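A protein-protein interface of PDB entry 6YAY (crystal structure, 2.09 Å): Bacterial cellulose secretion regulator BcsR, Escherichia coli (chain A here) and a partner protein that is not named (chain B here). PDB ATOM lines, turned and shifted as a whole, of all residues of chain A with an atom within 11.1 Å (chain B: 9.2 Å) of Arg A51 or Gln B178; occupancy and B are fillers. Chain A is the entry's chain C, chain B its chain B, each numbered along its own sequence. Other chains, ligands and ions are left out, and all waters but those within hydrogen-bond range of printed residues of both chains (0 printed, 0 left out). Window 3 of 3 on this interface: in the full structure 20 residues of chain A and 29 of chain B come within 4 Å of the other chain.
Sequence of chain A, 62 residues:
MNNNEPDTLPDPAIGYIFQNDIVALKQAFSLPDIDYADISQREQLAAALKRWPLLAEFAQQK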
ATOM      1  N   GLU A  43     -16.837   9.580 -25.170  1.00  0.00           N
ATOM      2  CA  GLU A  43     -17.475   9.771 -23.871  1.00  0.00           C
ATOM      3  C   GLU A  43     -16.725   9.050 -22.761  1.00  0.00           C
ATOM      4  O   GLU A  43     -16.755   9.490 -21.606  1.00  0.00           O
ATOM      5  CB  GLU A  43     -18.925   9.290 -23.926  1.00  0.00           C
ATOM      6  CG  GLU A  43     -19.710   9.810 -25.118  1.00  0.00           C
ATOM      7  CD  GLU A  43     -21.086   9.182 -25.230  1.00  0.00           C
ATOM      8  OE1 GLU A  43     -21.593   8.672 -24.209  1.00  0.00           O
ATOM      9  OE2 GLU A  43     -21.658   9.194 -26.340  1.00  0.00           O
ATOM     10  N   GLN A  44     -16.059   7.937 -23.083  1.00  0.00           N
ATOM     11  CA  GLN A  44     -15.286   7.229 -22.070  1.00  0.00           C
ATOM     12  C   GLN A  44     -14.113   8.065 -21.582  1.00  0.00           C
ATOM     13  O   GLN A  44     -13.739   7.986 -20.406  1.00  0.00           O
ATOM     14  CB  GLN A  44     -14.798   5.888 -22.619  1.00  0.00           C
ATOM     15  CG  GLN A  44     -15.915   4.920 -22.965  1.00  0.00           C
ATOM     16  CD  GLN A  44     -15.397   3.579 -23.443  1.00  0.00           C
ATOM     17  OE1 GLN A  44     -14.190   3.340 -23.472  1.00  0.00           O
ATOM     18  NE2 GLN A  44     -16.312   2.693 -23.824  1.00  0.00           N
ATOM     19  N   LEU A  45     -13.522   8.874 -22.465  1.00  0.00           N
ATOM     20  CA  LEU A  45     -12.456   9.771 -22.037  1.00  0.00           C
ATOM     21  C   LEU A  45     -12.993  10.913 -21.185  1.00  0.00           C
ATOM     22  O   LEU A  45     -12.263  11.456 -20.348  1.00  0.00           O
ATOM     23  CB  LEU A  45     -11.706  10.319 -23.251  1.00  0.00           C
ATOM     24  CG  LEU A  45     -10.925   9.292 -24.072  1.00  0.00           C
ATOM     25  CD1 LEU A  45     -10.145   9.975 -25.187  1.00  0.00           C
ATOM     26  CD2 LEU A  45      -9.997   8.485 -23.179  1.00  0.00           C
ATOM     27  N   ALA A  46     -14.261  11.286 -21.374  1.00  0.00           N
ATOM     28  CA  ALA A  46     -14.846  12.346 -20.558  1.00  0.00           C
ATOM     29  C   ALA A  46     -15.065  11.879 -19.125  1.00  0.00           C
ATOM     30  O   ALA A  46     -14.909  12.662 -18.181  1.00  0.00           O
ATOM     31  CB  ALA A  46     -16.159  12.823 -21.177  1.00  0.00           C
ATOM     32  N   ALA A  47     -15.428  10.607 -18.943  1.00  0.00           N
ATOM     33  CA  ALA A  47     -15.599  10.075 -17.596  1.00  0.00           C
ATOM     34  C   ALA A  47     -14.255   9.880 -16.908  1.00  0.00           C
ATOM     35  O   ALA A  47     -14.139  10.072 -15.691  1.00  0.00           O
ATOM     36  CB  ALA A  47     -16.375   8.759 -17.646  1.00  0.00           C
ATOM     37  N   ALA A  48     -13.228   9.495 -17.669  1.00  0.00           N
ATOM     38  CA  ALA A  48     -11.899   9.333 -17.089  1.00  0.00           C
ATOM     39  C   ALA A  48     -11.326  10.672 -16.643  1.00  0.00           C
ATOM     40  O   ALA A  48     -10.720  10.766 -15.570  1.00  0.00           O
ATOM     41  CB  ALA A  48     -10.966   8.651 -18.088  1.00  0.00           C
ATOM     42  N   LEU A  49     -11.503  11.719 -17.453  1.00  0.00           N
ATOM     43  CA  LEU A  49     -11.079  13.049 -17.030  1.00  0.00           C
ATOM     44  C   LEU A  49     -11.886  13.533 -15.833  1.00  0.00           C
ATOM     45  O   LEU A  49     -11.372  14.294 -15.007  1.00  0.00           O
ATOM     46  CB  LEU A  49     -11.205  14.043 -18.185  1.00  0.00           C
ATOM     47  CG  LEU A  49     -10.326  13.830 -19.418  1.00  0.00           C
ATOM     48  CD1 LEU A  49     -10.463  15.012 -20.361  1.00  0.00           C
ATOM     49  CD2 LEU A  49      -8.872  13.618 -19.026  1.00  0.00           C
ATOM     50  N   LYS A  50     -13.143  13.101 -15.726  1.00  0.00           N
ATOM     51  CA  LYS A  50     -13.966  13.478 -14.582  1.00  0.00           C
ATOM     52  C   LYS A  50     -13.426  12.880 -13.289  1.00  0.00           C
ATOM     53  O   LYS A  50     -13.412  13.548 -12.249  1.00  0.00           O
ATOM     54  CB  LYS A  50     -15.411  13.036 -14.815  1.00  0.00           C
ATOM     55  CG  LYS A  50     -16.262  12.979 -13.557  1.00  0.00           C
ATOM     56  CD  LYS A  50     -17.542  12.195 -13.797  1.00  0.00           C
ATOM     57  CE  LYS A  50     -17.243  10.812 -14.362  1.00  0.00           C
ATOM     58  NZ  LYS A  50     -16.291  10.043 -13.510  1.00  0.00           N
ATOM     59  N   ARG A  51     -12.971  11.626 -13.334  1.00  0.00           N
ATOM     60  CA  ARG A  51     -12.548  10.959 -12.107  1.00  0.00           C
ATOM     61  C   ARG A  51     -11.152  11.392 -11.671  1.00  0.00           C
ATOM     62  O   ARG A  51     -10.904  11.567 -10.473  1.00  0.00           O
ATOM     63  CB  ARG A  51     -12.597   9.441 -12.284  1.00  0.00           C
ATOM     64  CG  ARG A  51     -12.268   8.686 -11.005  1.00  0.00           C
ATOM     65  CD  ARG A  51     -12.429   7.182 -11.149  1.00  0.00           C
ATOM     66  NE  ARG A  51     -12.201   6.504  -9.875  1.00  0.00           N
ATOM     67  CZ  ARG A  51     -12.105   5.186  -9.729  1.00  0.00           C
ATOM     68  NH1 ARG A  51     -12.215   4.389 -10.784  1.00  0.00           N
ATOM     69  NH2 ARG A  51     -11.895   4.664  -8.528  1.00  0.00           N
ATOM     70  N   TRP A  52     -10.232  11.567 -12.615  1.00  0.00           N
ATOM     71  CA  TRP A  52      -8.841  11.831 -12.269  1.00  0.00           C
ATOM     72  C   TRP A  52      -8.493  13.289 -12.527  1.00  0.00           C
ATOM     73  O   TRP A  52      -8.341  13.687 -13.694  1.00  0.00           O
ATOM     74  CB  TRP A  52      -7.912  10.907 -13.059  1.00  0.00           C
ATOM     75  CG  TRP A  52      -8.317   9.474 -12.947  1.00  0.00           C
ATOM     76  CD1 TRP A  52      -8.736   8.657 -13.956  1.00  0.00           C
ATOM     77  CD2 TRP A  52      -8.377   8.695 -11.748  1.00  0.00           C
ATOM     78  NE1 TRP A  52      -9.037   7.412 -13.461  1.00  0.00           N
ATOM     79  CE2 TRP A  52      -8.827   7.409 -12.108  1.00  0.00           C
ATOM     80  CE3 TRP A  52      -8.087   8.957 -10.405  1.00  0.00           C
ATOM     81  CZ2 TRP A  52      -8.994   6.390 -11.175  1.00  0.00           C
ATOM     82  CZ3 TRP A  52      -8.253   7.944  -9.481  1.00  0.00           C
ATOM     83  CH2 TRP A  52      -8.705   6.678  -9.870  1.00  0.00           C
ATOM     84  N   PRO A  53      -8.360  14.115 -11.487  1.00  0.00           N
ATOM     85  CA  PRO A  53      -8.010  15.528 -11.714  1.00  0.00           C
ATOM     86  C   PRO A  53      -6.657  15.717 -12.376  1.00  0.00           C
ATOM     87  O   PRO A  53      -6.452  16.719 -13.073  1.00  0.00           O
ATOM     88  CB  PRO A  53      -8.032  16.124 -10.300  1.00  0.00           C
ATOM     89  CG  PRO A  53      -8.861  15.174  -9.490  1.00  0.00           C
ATOM     90  CD  PRO A  53      -8.599  13.822 -10.065  1.00  0.00           C
ATOM     91  N   LEU A  54      -5.722  14.786 -12.175  1.00  0.00           N
ATOM     92  CA  LEU A  54      -4.407  14.913 -12.795  1.00  0.00           C
ATOM     93  C   LEU A  54      -4.502  14.869 -14.315  1.00  0.00           C
ATOM     94  O   LEU A  54      -3.852  15.660 -15.008  1.00  0.00           O
ATOM     95  CB  LEU A  54      -3.482  13.808 -12.289  1.00  0.00           C
ATOM     96  CG  LEU A  54      -2.070  13.794 -12.872  1.00  0.00           C
ATOM     97  CD1 LEU A  54      -1.285  15.018 -12.417  1.00  0.00           C
ATOM     98  CD2 LEU A  54      -1.350  12.504 -12.493  1.00  0.00           C
ATOM     99  N   LEU A  55      -5.308  13.949 -14.853  1.00  0.00           N
ATOM    100  CA  LEU A  55      -5.457  13.860 -16.301  1.00  0.00           C
ATOM    101  C   LEU A  55      -6.197  15.071 -16.853  1.00  0.00           C
ATOM    102  O   LEU A  55      -5.854  15.580 -17.927  1.00  0.00           O
ATOM    103  CB  LEU A  55      -6.185  12.571 -16.679  1.00  0.00           C
ATOM    104  CG  LEU A  55      -5.613  11.267 -16.123  1.00  0.00           C
ATOM    105  CD1 LEU A  55      -6.410  10.078 -16.633  1.00  0.00           C
ATOM    106  CD2 LEU A  55      -4.148  11.124 -16.479  1.00  0.00           C
ATOM    107  N   ALA A  56      -7.213  15.548 -16.132  1.00  0.00           N
ATOM    108  CA  ALA A  56      -7.938  16.732 -16.578  1.00  0.00           C
ATOM    109  C   ALA A  56      -7.060  17.975 -16.530  1.00  0.00           C
ATOM    110  O   ALA A  56      -7.261  18.904 -17.322  1.00  0.00           O
ATOM    111  CB  ALA A  56      -9.193  16.931 -15.729  1.00  0.00           C
ATOM    112  N   GLU A  57      -6.085  18.007 -15.620  1.00  0.00           N
ATOM    113  CA  GLU A  57      -5.204  19.165 -15.516  1.00  0.00           C
ATOM    114  C   GLU A  57      -4.357  19.329 -16.773  1.00  0.00           C
ATOM    115  O   GLU A  57      -4.228  20.440 -17.298  1.00  0.00           O
ATOM    116  CB  GLU A  57      -4.316  19.033 -14.281  1.00  0.00           C
ATOM    117  CG  GLU A  57      -3.449  20.246 -14.010  1.00  0.00           C
ATOM    118  CD  GLU A  57      -2.558  20.060 -12.801  1.00  0.00           C
ATOM    119  OE1 GLU A  57      -2.515  18.934 -12.264  1.00  0.00           O
ATOM    120  OE2 GLU A  57      -1.900  21.039 -12.389  1.00  0.00           O
ATOM    121  N   ALA A  59      -5.080  17.931 -19.700  1.00  0.00           N
ATOM    122  CA  ALA A  59      -5.915  17.917 -20.897  1.00  0.00           C
ATOM    123  C   ALA A  59      -6.389  19.316 -21.270  1.00  0.00           C
ATOM    124  O   ALA A  59      -6.415  19.673 -22.453  1.00  0.00           O
ATOM    125  CB  ALA A  59      -7.106  16.984 -20.688  1.00  0.00           C
ATOM    126  N   VAL B 149       2.439   2.391 -18.138  1.00  0.00           N
ATOM    127  CA  VAL B 149       1.230   3.208 -18.148  1.00  0.00           C
ATOM    128  C   VAL B 149       0.793   3.482 -16.716  1.00  0.00           C
ATOM    129  O   VAL B 149       0.057   2.690 -16.116  1.00  0.00           O
ATOM    130  CB  VAL B 149       0.099   2.553 -18.954  1.00  0.00           C
ATOM    131  CG1 VAL B 149      -1.073   3.513 -19.065  1.00  0.00           C
ATOM    132  CG2 VAL B 149       0.601   2.159 -20.335  1.00  0.00           C
ATOM    133  N   PHE B 173       2.219  -3.650 -19.198  1.00  0.00           N
ATOM    134  CA  PHE B 173       0.766  -3.547 -19.195  1.00  0.00           C
ATOM    135  C   PHE B 173       0.182  -4.732 -18.433  1.00  0.00           C
ATOM    136  O   PHE B 173       0.591  -5.878 -18.635  1.00  0.00           O
ATOM    137  CB  PHE B 173       0.236  -3.499 -20.629  1.00  0.00           C
ATOM    138  CG  PHE B 173      -1.065  -2.760 -20.770  1.00  0.00           C
ATOM    139  CD1 PHE B 173      -1.101  -1.376 -20.715  1.00  0.00           C
ATOM    140  CD2 PHE B 173      -2.250  -3.448 -20.969  1.00  0.00           C
ATOM    141  CE1 PHE B 173      -2.297  -0.694 -20.847  1.00  0.00           C
ATOM    142  CE2 PHE B 173      -3.445  -2.771 -21.103  1.00  0.00           C
ATOM    143  CZ  PHE B 173      -3.468  -1.393 -21.045  1.00  0.00           C
ATOM    144  N   ARG B 174      -0.796  -4.444 -17.573  1.00  0.00           N
ATOM    145  CA  ARG B 174      -1.253  -5.374 -16.552  1.00  0.00           C
ATOM    146  C   ARG B 174      -2.777  -5.415 -16.528  1.00  0.00           C
ATOM    147  O   ARG B 174      -3.450  -4.482 -16.970  1.00  0.00           O
ATOM    148  CB  ARG B 174      -0.706  -4.960 -15.174  1.00  0.00           C
ATOM    149  CG  ARG B 174      -0.819  -6.004 -14.076  1.00  0.00           C
ATOM    150  CD  ARG B 174      -0.110  -5.539 -12.807  1.00  0.00           C
ATOM    151  NE  ARG B 174      -0.553  -4.212 -12.385  1.00  0.00           N
ATOM    152  CZ  ARG B 174      -1.644  -3.984 -11.661  1.00  0.00           C
ATOM    153  NH1 ARG B 174      -2.412  -4.995 -11.276  1.00  0.00           N
ATOM    154  NH2 ARG B 174      -1.971  -2.744 -11.324  1.00  0.00           N
ATOM    155  N   ILE B 175      -3.319  -6.524 -16.006  1.00  0.00           N
ATOM    156  CA  ILE B 175      -4.743  -6.640 -15.713  1.00  0.00           C
ATOM    157  C   ILE B 175      -4.972  -6.110 -14.306  1.00  0.00           C
ATOM    158  O   ILE B 175      -4.080  -6.160 -13.453  1.00  0.00           O
ATOM    159  CB  ILE B 175      -5.226  -8.101 -15.838  1.00  0.00           C
ATOM    160  CG1 ILE B 175      -4.735  -8.730 -17.141  1.00  0.00           C
ATOM    161  CG2 ILE B 175      -6.757  -8.193 -15.729  1.00  0.00           C
ATOM    162  CD1 ILE B 175      -5.365  -8.160 -18.384  1.00  0.00           C
ATOM    163  N   GLY B 176      -6.173  -5.585 -14.061  1.00  0.00           N
ATOM    164  CA  GLY B 176      -6.599  -5.247 -12.717  1.00  0.00           C
ATOM    165  C   GLY B 176      -6.349  -3.825 -12.275  1.00  0.00           C
ATOM    166  O   GLY B 176      -6.321  -3.567 -11.066  1.00  0.00           O
ATOM    167  N   SER B 177      -6.176  -2.888 -13.202  1.00  0.00           N
ATOM    168  CA  SER B 177      -5.892  -1.499 -12.857  1.00  0.00           C
ATOM    169  C   SER B 177      -6.785  -0.590 -13.687  1.00  0.00           C
ATOM    170  O   SER B 177      -6.564  -0.428 -14.891  1.00  0.00           O
ATOM    171  CB  SER B 177      -4.417  -1.163 -13.080  1.00  0.00           C
ATOM    172  OG  SER B 177      -4.155   0.192 -12.758  1.00  0.00           O
ATOM    173  N   GLN B 178      -7.780   0.014 -13.038  1.00  0.00           N
ATOM    174  CA  GLN B 178      -8.662   0.944 -13.736  1.00  0.00           C
ATOM    175  C   GLN B 178      -7.922   2.210 -14.151  1.00  0.00           C
ATOM    176  O   GLN B 178      -8.114   2.706 -15.269  1.00  0.00           O
ATOM    177  CB  GLN B 178      -9.860   1.294 -12.855  1.00  0.00           C
ATOM    178  CG  GLN B 178     -10.845   2.247 -13.511  1.00  0.00           C
ATOM    179  CD  GLN B 178     -11.474   1.660 -14.763  1.00  0.00           C
ATOM    180  OE1 GLN B 178     -11.777   0.468 -14.818  1.00  0.00           O
ATOM    181  NE2 GLN B 178     -11.667   2.495 -15.777  1.00  0.00           N
ATOM    182  N   VAL B 179      -7.075   2.754 -13.273  1.00  0.00           N
ATOM    183  CA  VAL B 179      -6.398   4.005 -13.603  1.00  0.00           C
ATOM    184  C   VAL B 179      -5.442   3.803 -14.776  1.00  0.00           C
ATOM    185  O   VAL B 179      -5.304   4.683 -15.633  1.00  0.00           O
ATOM    186  CB  VAL B 179      -5.688   4.594 -12.366  1.00  0.00           C
ATOM    187  CG1 VAL B 179      -4.553   3.694 -11.879  1.00  0.00           C
ATOM    188  CG2 VAL B 179      -5.170   5.993 -12.669  1.00  0.00           C
ATOM    189  N   GLN B 180      -4.788   2.638 -14.853  1.00  0.00           N
ATOM    190  CA  GLN B 180      -3.945   2.351 -16.011  1.00  0.00           C
ATOM    191  C   GLN B 180      -4.761   2.346 -17.296  1.00  0.00           C
ATOM    192  O   GLN B 180      -4.321   2.874 -18.324  1.00  0.00           O
ATOM    193  CB  GLN B 180      -3.231   1.009 -15.838  1.00  0.00           C
ATOM    194  CG  GLN B 180      -2.483   0.558 -17.083  1.00  0.00           C
ATOM    195  CD  GLN B 180      -2.328  -0.950 -17.169  1.00  0.00           C
ATOM    196  OE1 GLN B 180      -1.276  -1.497 -16.843  1.00  0.00           O
ATOM    197  NE2 GLN B 180      -3.379  -1.629 -17.613  1.00  0.00           N
ATOM    198  N   ASP B 181      -5.959   1.760 -17.256  1.00  0.00           N
ATOM    199  CA  ASP B 181      -6.788   1.703 -18.453  1.00  0.00           C
ATOM    200  C   ASP B 181      -7.305   3.080 -18.848  1.00  0.00           C
ATOM    201  O   ASP B 181      -7.455   3.361 -20.043  1.00  0.00           O
ATOM    202  CB  ASP B 181      -7.945   0.730 -18.237  1.00  0.00           C
ATOM    203  CG  ASP B 181      -7.466  -0.680 -17.949  1.00  0.00           C
ATOM    204  OD1 ASP B 181      -6.311  -0.996 -18.315  1.00  0.00           O
ATOM    205  OD2 ASP B 181      -8.234  -1.469 -17.359  1.00  0.00           O
ATOM    206  N   ASP B 182      -7.576   3.950 -17.871  1.00  0.00           N
ATOM    207  CA  ASP B 182      -7.996   5.312 -18.191  1.00  0.00           C
ATOM    208  C   ASP B 182      -6.865   6.095 -18.849  1.00  0.00           C
ATOM    209  O   ASP B 182      -7.074   6.781 -19.857  1.00  0.00           O
ATOM    210  CB  ASP B 182      -8.481   6.025 -16.929  1.00  0.00           C
ATOM    211  CG  ASP B 182      -9.828   5.516 -16.449  1.00  0.00           C
ATOM    212  OD1 ASP B 182     -10.590   4.974 -17.277  1.00  0.00           O
ATOM    213  OD2 ASP B 182     -10.124   5.666 -15.244  1.00  0.00           O
ATOM    214  N   ILE B 183      -5.655   6.003 -18.291  1.00  0.00           N
ATOM    215  CA  ILE B 183      -4.506   6.677 -18.889  1.00  0.00           C
ATOM    216  C   ILE B 183      -4.233   6.134 -20.289  1.00  0.00           C
ATOM    217  O   ILE B 183      -3.959   6.896 -21.223  1.00  0.00           O
ATOM    218  CB  ILE B 183      -3.273   6.540 -17.977  1.00  0.00           C
ATOM    219  CG1 ILE B 183      -3.525   7.212 -16.625  1.00  0.00           C
ATOM    220  CG2 ILE B 183      -2.037   7.126 -18.649  1.00  0.00           C
ATOM    221  CD1 ILE B 183      -2.402   7.005 -15.630  1.00  0.00           C
ATOM    222  N   TYR B 184      -4.315   4.809 -20.456  1.00  0.00           N
ATOM    223  CA  TYR B 184      -4.000   4.200 -21.748  1.00  0.00           C
ATOM    224  C   TYR B 184      -4.969   4.656 -22.832  1.00  0.00           C
ATOM    225  O   TYR B 184      -4.549   4.996 -23.944  1.00  0.00           O
ATOM    226  CB  TYR B 184      -4.006   2.675 -21.630  1.00  0.00           C
ATOM    227  CG  TYR B 184      -3.840   1.965 -22.956  1.00  0.00           C
ATOM    228  CD1 TYR B 184      -2.667   2.088 -23.691  1.00  0.00           C
ATOM    229  CD2 TYR B 184      -4.854   1.167 -23.471  1.00  0.00           C
ATOM    230  CE1 TYR B 184      -2.511   1.443 -24.902  1.00  0.00           C
ATOM    231  CE2 TYR B 184      -4.706   0.516 -24.682  1.00  0.00           C
ATOM    232  CZ  TYR B 184      -3.532   0.659 -25.394  1.00  0.00           C
ATOM    233  OH  TYR B 184      -3.379   0.015 -26.602  1.00  0.00           O
ATOM    234  N   GLN B 185      -6.269   4.665 -22.530  1.00  0.00           N
ATOM    235  CA  GLN B 185      -7.240   5.163 -23.500  1.00  0.00           C
ATOM    236  C   GLN B 185      -7.001   6.632 -23.817  1.00  0.00           C
ATOM    237  O   GLN B 185      -7.213   7.064 -24.956  1.00  0.00           O
ATOM    238  CB  GLN B 185      -8.663   4.951 -22.980  1.00  0.00           C
ATOM    239  CG  GLN B 185      -9.053   3.490 -22.796  1.00  0.00           C
ATOM    240  CD  GLN B 185      -9.070   2.716 -24.101  1.00  0.00           C
ATOM    241  OE1 GLN B 185      -9.328   3.276 -25.167  1.00  0.00           O
ATOM    242  NE2 GLN B 185      -8.793   1.420 -24.021  1.00  0.00           N
ATOM    243  N   LEU B 186      -6.562   7.414 -22.828  1.00  0.00           N
ATOM    244  CA  LEU B 186      -6.211   8.805 -23.090  1.00  0.00           C
ATOM    245  C   LEU B 186      -4.998   8.903 -24.007  1.00  0.00           C
ATOM    246  O   LEU B 186      -4.949   9.769 -24.888  1.00  0.00           O
ATOM    247  CB  LEU B 186      -5.954   9.537 -21.773  1.00  0.00           C
ATOM    248  CG  LEU B 186      -5.523  11.004 -21.839  1.00  0.00           C
ATOM    249  CD1 LEU B 186      -6.481  11.814 -22.694  1.00  0.00           C
ATOM    250  CD2 LEU B 186      -5.439  11.589 -20.437  1.00  0.00           C
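The indole nitrogen (NE1) of Trp A52 sits at hydrogen-bond distance from the side-chain carboxylate (OD2) of Asp B182 (2.7 Å).
OD1 of Asp B182 is in hydrogen-bond range of NE2 of Gln B178 (3.1 Å).
Among the printed residues, merely in contact across the chains: Leu A45 with Gln B185 (3.6 Å), Leu A45 with Leu B186 (3.6 Å), Ala A48 with Asp B182 (3.7 Å), Arg A51 with Gln B178 (3.7 Å), Trp A52 with Val B179 (3.9 Å), Leu A55 with Ile B183 (3.96 Å) and Leu A55 with Leu B186 (3.96 Å).
Printed residues of chain B within 4 Å of Ala A48: Asp B182. Of chain B, only Gln B178 (3.7 Å) comes within 4 Å of Arg A51. Trp A52 touches two residues of chain B. No residue of chain A comes within 4 Å of Gly B176. No residue of chain A comes within 4 Å of Ser B177. Of the printed residues of chain A, Gln B178 touches Arg A51 (3.7 Å). Val B179 touches just one residue of chain A: Trp A52 (3.9 Å). Asp B182 touches just these residues of chain A: Ala A48 (3.7 Å) and Trp A52 (2.7 Å). Printed residues of chain A within 4 Å of Ile B183: Leu A55 (3.96 Å). Printed residues of chain A within 4 Å of Leu B186: Leu A45 (3.6 Å) and Leu A55 (3.96 Å). The nearest printed residue of chain A that does not touch Gln B185 is Gln A44 (5.1 Å).
Of the 16 printed residues of chain A, 5 touch a printed residue of chain B. Along chain A the printed residues that touch a printed residue of chain B span positions 45 to 55. Hydrophobic or aromatic side chains of chain B within 4 Å of the printed part of chain A: Val B179, Ile B183 and Leu B186. Among the printed residues, 8 pairs touch across the chains.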
